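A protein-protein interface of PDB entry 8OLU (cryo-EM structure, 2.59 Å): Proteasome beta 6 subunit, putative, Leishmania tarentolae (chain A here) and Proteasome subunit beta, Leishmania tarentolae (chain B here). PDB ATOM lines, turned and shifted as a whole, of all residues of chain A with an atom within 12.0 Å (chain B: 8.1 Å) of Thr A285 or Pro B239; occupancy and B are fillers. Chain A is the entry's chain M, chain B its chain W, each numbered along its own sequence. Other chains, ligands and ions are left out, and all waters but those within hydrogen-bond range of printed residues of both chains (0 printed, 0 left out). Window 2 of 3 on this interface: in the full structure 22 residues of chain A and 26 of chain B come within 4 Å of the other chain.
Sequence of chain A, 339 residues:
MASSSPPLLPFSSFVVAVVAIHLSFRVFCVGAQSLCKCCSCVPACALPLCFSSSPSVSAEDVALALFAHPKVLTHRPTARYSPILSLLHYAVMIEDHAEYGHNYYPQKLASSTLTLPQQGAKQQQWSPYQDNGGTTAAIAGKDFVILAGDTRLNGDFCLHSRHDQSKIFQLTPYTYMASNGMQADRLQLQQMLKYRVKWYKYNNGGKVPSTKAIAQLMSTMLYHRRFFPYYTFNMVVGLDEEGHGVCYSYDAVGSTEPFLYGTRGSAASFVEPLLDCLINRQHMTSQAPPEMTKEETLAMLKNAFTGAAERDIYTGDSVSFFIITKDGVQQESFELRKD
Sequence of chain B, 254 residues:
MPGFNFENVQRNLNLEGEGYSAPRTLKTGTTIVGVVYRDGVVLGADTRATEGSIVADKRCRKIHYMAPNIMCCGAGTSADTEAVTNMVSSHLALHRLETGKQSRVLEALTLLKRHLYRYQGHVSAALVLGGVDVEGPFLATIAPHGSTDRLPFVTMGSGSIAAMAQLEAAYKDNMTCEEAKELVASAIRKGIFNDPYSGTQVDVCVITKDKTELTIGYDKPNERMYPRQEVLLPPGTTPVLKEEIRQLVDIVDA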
ATOM      1  N   ASP A 276      -2.494  -5.184   7.446  1.00  0.00           N
ATOM      2  CA  ASP A 276      -3.360  -6.147   6.793  1.00  0.00           C
ATOM      3  C   ASP A 276      -2.530  -6.814   5.732  1.00  0.00           C
ATOM      4  O   ASP A 276      -2.333  -7.999   5.782  1.00  0.00           O
ATOM      5  CB  ASP A 276      -4.603  -5.548   6.134  1.00  0.00           C
ATOM      6  CG  ASP A 276      -5.689  -5.034   7.079  1.00  0.00           C
ATOM      7  OD1 ASP A 276      -5.605  -5.363   8.292  1.00  0.00           O
ATOM      8  OD2 ASP A 276      -6.612  -4.279   6.594  1.00  0.00           O
ATOM      9  N   CYS A 277      -1.927  -6.026   4.867  1.00  0.00           N
ATOM     10  CA  CYS A 277      -1.215  -6.550   3.717  1.00  0.00           C
ATOM     11  C   CYS A 277      -0.032  -7.460   4.096  1.00  0.00           C
ATOM     12  O   CYS A 277       0.272  -8.363   3.348  1.00  0.00           O
ATOM     13  CB  CYS A 277      -0.783  -5.368   2.863  1.00  0.00           C
ATOM     14  SG  CYS A 277       0.181  -5.727   1.371  1.00  0.00           S
ATOM     15  N   LEU A 278       0.694  -7.235   5.181  1.00  0.00           N
ATOM     16  CA  LEU A 278       1.991  -7.898   5.315  1.00  0.00           C
ATOM     17  C   LEU A 278       1.889  -9.086   6.252  1.00  0.00           C
ATOM     18  O   LEU A 278       2.679 -10.019   6.158  1.00  0.00           O
ATOM     19  CB  LEU A 278       3.049  -6.914   5.832  1.00  0.00           C
ATOM     20  CG  LEU A 278       3.166  -5.639   4.992  1.00  0.00           C
ATOM     21  CD1 LEU A 278       4.220  -4.684   5.544  1.00  0.00           C
ATOM     22  CD2 LEU A 278       3.447  -6.006   3.536  1.00  0.00           C
ATOM     23  N   ILE A 279       0.912  -9.003   7.146  1.00  0.00           N
ATOM     24  CA  ILE A 279       0.555 -10.087   8.028  1.00  0.00           C
ATOM     25  C   ILE A 279      -0.343 -11.092   7.325  1.00  0.00           C
ATOM     26  O   ILE A 279       0.023 -12.257   7.299  1.00  0.00           O
ATOM     27  CB  ILE A 279      -0.095  -9.486   9.264  1.00  0.00           C
ATOM     28  CG1 ILE A 279       0.879  -8.492   9.902  1.00  0.00           C
ATOM     29  CG2 ILE A 279      -0.550 -10.589  10.203  1.00  0.00           C
ATOM     30  CD1 ILE A 279       0.460  -7.932  11.230  1.00  0.00           C
ATOM     31  N   ASN A 280      -1.484 -10.658   6.756  1.00  0.00           N
ATOM     32  CA  ASN A 280      -2.488 -11.591   6.249  1.00  0.00           C
ATOM     33  C   ASN A 280      -2.242 -11.975   4.797  1.00  0.00           C
ATOM     34  O   ASN A 280      -2.606 -13.073   4.391  1.00  0.00           O
ATOM     35  CB  ASN A 280      -3.927 -11.093   6.413  1.00  0.00           C
ATOM     36  CG  ASN A 280      -4.265 -10.842   7.865  1.00  0.00           C
ATOM     37  OD1 ASN A 280      -4.963  -9.884   8.196  1.00  0.00           O
ATOM     38  ND2 ASN A 280      -3.797 -11.722   8.740  1.00  0.00           N
ATOM     39  N   ARG A 281      -1.744 -11.048   4.002  1.00  0.00           N
ATOM     40  CA  ARG A 281      -1.339 -11.324   2.625  1.00  0.00           C
ATOM     41  C   ARG A 281      -2.447 -11.942   1.764  1.00  0.00           C
ATOM     42  O   ARG A 281      -2.148 -12.720   0.857  1.00  0.00           O
ATOM     43  CB  ARG A 281      -0.100 -12.211   2.644  1.00  0.00           C
ATOM     44  CG  ARG A 281       0.879 -11.823   3.739  1.00  0.00           C
ATOM     45  CD  ARG A 281       2.159 -12.622   3.697  1.00  0.00           C
ATOM     46  NE  ARG A 281       2.869 -12.523   2.427  1.00  0.00           N
ATOM     47  CZ  ARG A 281       3.972 -11.803   2.235  1.00  0.00           C
ATOM     48  NH1 ARG A 281       4.227 -10.732   2.980  1.00  0.00           N
ATOM     49  NH2 ARG A 281       4.785 -12.143   1.246  1.00  0.00           N
ATOM     50  N   GLN A 282      -3.693 -11.482   1.939  1.00  0.00           N
ATOM     51  CA  GLN A 282      -4.820 -12.156   1.323  1.00  0.00           C
ATOM     52  C   GLN A 282      -4.846 -11.943  -0.190  1.00  0.00           C
ATOM     53  O   GLN A 282      -5.442 -12.752  -0.898  1.00  0.00           O
ATOM     54  CB  GLN A 282      -6.137 -11.829   2.026  1.00  0.00           C
ATOM     55  CG  GLN A 282      -6.688 -10.441   1.766  1.00  0.00           C
ATOM     56  CD  GLN A 282      -8.195 -10.385   1.911  1.00  0.00           C
ATOM     57  OE1 GLN A 282      -8.933 -11.097   1.224  1.00  0.00           O
ATOM     58  NE2 GLN A 282      -8.655  -9.499   2.784  1.00  0.00           N
ATOM     59  N   HIS A 283      -4.096 -10.969  -0.713  1.00  0.00           N
ATOM     60  CA  HIS A 283      -4.039 -10.773  -2.151  1.00  0.00           C
ATOM     61  C   HIS A 283      -2.710 -11.209  -2.739  1.00  0.00           C
ATOM     62  O   HIS A 283      -2.391 -10.832  -3.864  1.00  0.00           O
ATOM     63  CB  HIS A 283      -4.353  -9.305  -2.480  1.00  0.00           C
ATOM     64  CG  HIS A 283      -5.758  -8.924  -2.112  1.00  0.00           C
ATOM     65  ND1 HIS A 283      -6.861  -9.458  -2.748  1.00  0.00           N
ATOM     66  CD2 HIS A 283      -6.204  -8.111  -1.105  1.00  0.00           C
ATOM     67  CE1 HIS A 283      -7.955  -9.007  -2.160  1.00  0.00           C
ATOM     68  NE2 HIS A 283      -7.573  -8.158  -1.149  1.00  0.00           N
ATOM     69  N   MET A 284      -1.948 -12.030  -2.011  1.00  0.00           N
ATOM     70  CA  MET A 284      -0.687 -12.543  -2.542  1.00  0.00           C
ATOM     71  C   MET A 284      -0.784 -14.048  -2.834  1.00  0.00           C
ATOM     72  O   MET A 284      -1.239 -14.811  -1.979  1.00  0.00           O
ATOM     73  CB  MET A 284       0.416 -12.244  -1.524  1.00  0.00           C
ATOM     74  CG  MET A 284       0.880 -10.802  -1.570  1.00  0.00           C
ATOM     75  SD  MET A 284       1.932 -10.445  -0.160  1.00  0.00           S
ATOM     76  CE  MET A 284       1.628  -8.702   0.146  1.00  0.00           C
ATOM     77  N   THR A 285      -0.392 -14.460  -4.053  1.00  0.00           N
ATOM     78  CA  THR A 285      -0.391 -15.866  -4.463  1.00  0.00           C
ATOM     79  C   THR A 285       0.733 -16.620  -3.739  1.00  0.00           C
ATOM     80  O   THR A 285       0.494 -17.652  -3.104  1.00  0.00           O
ATOM     81  CB  THR A 285      -0.248 -16.050  -5.988  1.00  0.00           C
ATOM     82  OG1 THR A 285       0.956 -15.436  -6.454  1.00  0.00           O
ATOM     83  CG2 THR A 285      -1.407 -15.484  -6.781  1.00  0.00           C
ATOM     84  N   SER A 286       1.957 -16.090  -3.868  1.00  0.00           N
ATOM     85  CA  SER A 286       3.069 -16.380  -2.975  1.00  0.00           C
ATOM     86  C   SER A 286       2.578 -16.920  -1.628  1.00  0.00           C
ATOM     87  O   SER A 286       1.809 -16.260  -0.931  1.00  0.00           O
ATOM     88  CB  SER A 286       3.893 -15.130  -2.781  1.00  0.00           C
ATOM     89  OG  SER A 286       5.065 -15.425  -2.042  1.00  0.00           O
ATOM     90  N   GLN A 287       3.053 -18.121  -1.261  1.00  0.00           N
ATOM     91  CA  GLN A 287       2.681 -18.783  -0.016  1.00  0.00           C
ATOM     92  C   GLN A 287       3.156 -17.945   1.177  1.00  0.00           C
ATOM     93  O   GLN A 287       4.271 -17.421   1.156  1.00  0.00           O
ATOM     94  CB  GLN A 287       3.272 -20.201  -0.011  1.00  0.00           C
ATOM     95  CG  GLN A 287       3.281 -20.892   1.352  1.00  0.00           C
ATOM     96  CD  GLN A 287       4.481 -21.789   1.557  1.00  0.00           C
ATOM     97  OE1 GLN A 287       5.618 -21.420   1.260  1.00  0.00           O
ATOM     98  NE2 GLN A 287       4.239 -22.978   2.084  1.00  0.00           N
ATOM     99  N   ALA A 288       2.300 -17.854   2.214  1.00  0.00           N
ATOM    100  CA  ALA A 288       2.526 -17.029   3.399  1.00  0.00           C
ATOM    101  C   ALA A 288       3.870 -17.380   4.051  1.00  0.00           C
ATOM    102  O   ALA A 288       4.113 -18.553   4.329  1.00  0.00           O
ATOM    103  CB  ALA A 288       1.368 -17.212   4.366  1.00  0.00           C
ATOM    104  N   PRO A 289       4.783 -16.407   4.334  1.00  0.00           N
ATOM    105  CA  PRO A 289       6.087 -16.719   4.930  1.00  0.00           C
ATOM    106  C   PRO A 289       5.913 -17.241   6.363  1.00  0.00           C
ATOM    107  O   PRO A 289       4.788 -17.392   6.847  1.00  0.00           O
ATOM    108  CB  PRO A 289       6.874 -15.392   4.827  1.00  0.00           C
ATOM    109  CG  PRO A 289       5.816 -14.314   4.806  1.00  0.00           C
ATOM    110  CD  PRO A 289       4.606 -14.955   4.150  1.00  0.00           C
ATOM    111  N   PRO B 234       7.390 -10.243  -5.844  1.00  0.00           N
ATOM    112  CA  PRO B 234       7.896 -10.694  -7.145  1.00  0.00           C
ATOM    113  C   PRO B 234       6.815 -10.839  -8.201  1.00  0.00           C
ATOM    114  O   PRO B 234       5.745 -11.355  -7.909  1.00  0.00           O
ATOM    115  CB  PRO B 234       8.436 -12.104  -6.867  1.00  0.00           C
ATOM    116  CG  PRO B 234       7.669 -12.571  -5.628  1.00  0.00           C
ATOM    117  CD  PRO B 234       7.353 -11.319  -4.832  1.00  0.00           C
ATOM    118  N   PRO B 235       7.054 -10.430  -9.463  1.00  0.00           N
ATOM    119  CA  PRO B 235       6.051 -10.607 -10.520  1.00  0.00           C
ATOM    120  C   PRO B 235       5.189 -11.871 -10.400  1.00  0.00           C
ATOM    121  O   PRO B 235       5.677 -12.933 -10.007  1.00  0.00           O
ATOM    122  CB  PRO B 235       6.938 -10.615 -11.773  1.00  0.00           C
ATOM    123  CG  PRO B 235       8.037  -9.613 -11.424  1.00  0.00           C
ATOM    124  CD  PRO B 235       8.275  -9.754  -9.932  1.00  0.00           C
ATOM    125  N   GLY B 236       3.895 -11.722 -10.733  1.00  0.00           N
ATOM    126  CA  GLY B 236       2.900 -12.779 -10.645  1.00  0.00           C
ATOM    127  C   GLY B 236       2.295 -12.898  -9.243  1.00  0.00           C
ATOM    128  O   GLY B 236       1.376 -13.693  -9.029  1.00  0.00           O
ATOM    129  N   THR B 237       2.824 -12.112  -8.293  1.00  0.00           N
ATOM    130  CA  THR B 237       2.375 -12.129  -6.905  1.00  0.00           C
ATOM    131  C   THR B 237       0.904 -11.750  -6.791  1.00  0.00           C
ATOM    132  O   THR B 237       0.207 -12.245  -5.906  1.00  0.00           O
ATOM    133  CB  THR B 237       3.271 -11.245  -6.018  1.00  0.00           C
ATOM    134  OG1 THR B 237       4.160 -12.105  -5.291  1.00  0.00           O
ATOM    135  CG2 THR B 237       2.540 -10.417  -4.992  1.00  0.00           C
ATOM    136  N   THR B 238       0.441 -10.836  -7.646  1.00  0.00           N
ATOM    137  CA  THR B 238      -0.919 -10.346  -7.523  1.00  0.00           C
ATOM    138  C   THR B 238      -1.772 -11.052  -8.572  1.00  0.00           C
ATOM    139  O   THR B 238      -1.409 -11.086  -9.741  1.00  0.00           O
ATOM    140  CB  THR B 238      -0.984  -8.811  -7.590  1.00  0.00           C
ATOM    141  OG1 THR B 238      -0.095  -8.200  -6.649  1.00  0.00           O
ATOM    142  CG2 THR B 238      -2.379  -8.304  -7.292  1.00  0.00           C
ATOM    143  N   PRO B 239      -2.934 -11.629  -8.179  1.00  0.00           N
ATOM    144  CA  PRO B 239      -3.801 -12.374  -9.095  1.00  0.00           C
ATOM    145  C   PRO B 239      -4.495 -11.498 -10.120  1.00  0.00           C
ATOM    146  O   PRO B 239      -5.235 -10.577  -9.785  1.00  0.00           O
ATOM    147  CB  PRO B 239      -4.886 -13.007  -8.218  1.00  0.00           C
ATOM    148  CG  PRO B 239      -4.357 -12.871  -6.788  1.00  0.00           C
ATOM    149  CD  PRO B 239      -3.482 -11.628  -6.818  1.00  0.00           C
ATOM    150  N   VAL B 240      -4.214 -11.830 -11.375  1.00  0.00           N
ATOM    151  CA  VAL B 240      -4.739 -11.132 -12.522  1.00  0.00           C
ATOM    152  C   VAL B 240      -5.746 -12.046 -13.195  1.00  0.00           C
ATOM    153  O   VAL B 240      -5.581 -13.265 -13.179  1.00  0.00           O
ATOM    154  CB  VAL B 240      -3.586 -10.705 -13.445  1.00  0.00           C
ATOM    155  CG1 VAL B 240      -4.074 -10.169 -14.783  1.00  0.00           C
ATOM    156  CG2 VAL B 240      -2.710  -9.663 -12.757  1.00  0.00           C
ATOM    157  N   LEU B 241      -6.805 -11.420 -13.714  1.00  0.00           N
ATOM    158  CA  LEU B 241      -7.935 -12.091 -14.318  1.00  0.00           C
ATOM    159  C   LEU B 241      -7.819 -12.033 -15.834  1.00  0.00           C
ATOM    160  O   LEU B 241      -8.095 -13.011 -16.522  1.00  0.00           O
ATOM    161  CB  LEU B 241      -9.227 -11.390 -13.892  1.00  0.00           C
ATOM    162  CG  LEU B 241      -9.675 -11.560 -12.442  1.00  0.00           C
ATOM    163  CD1 LEU B 241     -11.133 -11.078 -12.284  1.00  0.00           C
ATOM    164  CD2 LEU B 241      -9.501 -13.010 -11.952  1.00  0.00           C
ATOM    165  N   LYS B 242      -7.523 -10.837 -16.332  1.00  0.00           N
ATOM    166  CA  LYS B 242      -7.356 -10.593 -17.751  1.00  0.00           C
ATOM    167  C   LYS B 242      -6.214  -9.609 -17.915  1.00  0.00           C
ATOM    168  O   LYS B 242      -5.817  -8.951 -16.959  1.00  0.00           O
ATOM    169  CB  LYS B 242      -8.615 -10.009 -18.386  1.00  0.00           C
ATOM    170  CG  LYS B 242      -9.870 -10.849 -18.231  1.00  0.00           C
ATOM    171  CD  LYS B 242     -11.097 -10.224 -18.913  1.00  0.00           C
ATOM    172  CE  LYS B 242     -12.023 -11.266 -19.512  1.00  0.00           C
ATOM    173  NZ  LYS B 242     -13.368 -10.715 -19.789  1.00  0.00           N
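OG1 of Thr A285 sits at hydrogen-bond distance from O of Gly B236, 3.1 Å away. The backbone NH of Thr A285 sits at hydrogen-bond distance from the backbone carbonyl oxygen of Thr B237 (2.9 Å).
SD of Met A284 lies close to NE of Arg A281, at 3.4 Å. The side-chain hydroxyl (OG1) of Thr B237 sits close to the backbone carbonyl oxygen (O) of Pro B234 (3.2 Å).
Among the printed residues, merely in contact across the chains: His A283 with Pro B239, Met A284 with Thr B237, His A283 with Thr B237, Ser A286 with Thr B237, Thr A285 with Pro B239 and His A283 with Thr B238.
Of chain A, only His A283 and Thr A285 come within 4 Å of Pro B239. Of chain A, only Thr A285 (3.1 Å) comes within 4 Å of Gly B236. Thr B238 touches one residue of chain A. No residue of chain A comes within 4 Å of Val B240. Printed residues of chain B within 4 Å of His A283: Thr B237, Thr B238 and Pro B239. Of the printed residues of chain B, Ser A286 touches Thr B237. Printed residues of chain B within 4 Å of Met A284: Thr B237 (3.5 Å). Leu A278 touches none of the printed residues of chain B. Pro A289 touches none of the printed residues of chain B. The nearest printed residue of chain B that does not touch Met A284 is Pro B239 (5.1 Å).
Hydrophobic or aromatic side chains of chain A that line the printed part of chain B: Met A284. Of the 9 printed residues of chain B, 4 touch a printed residue of chain A. Among the printed residues, 8 pairs touch across the chains.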
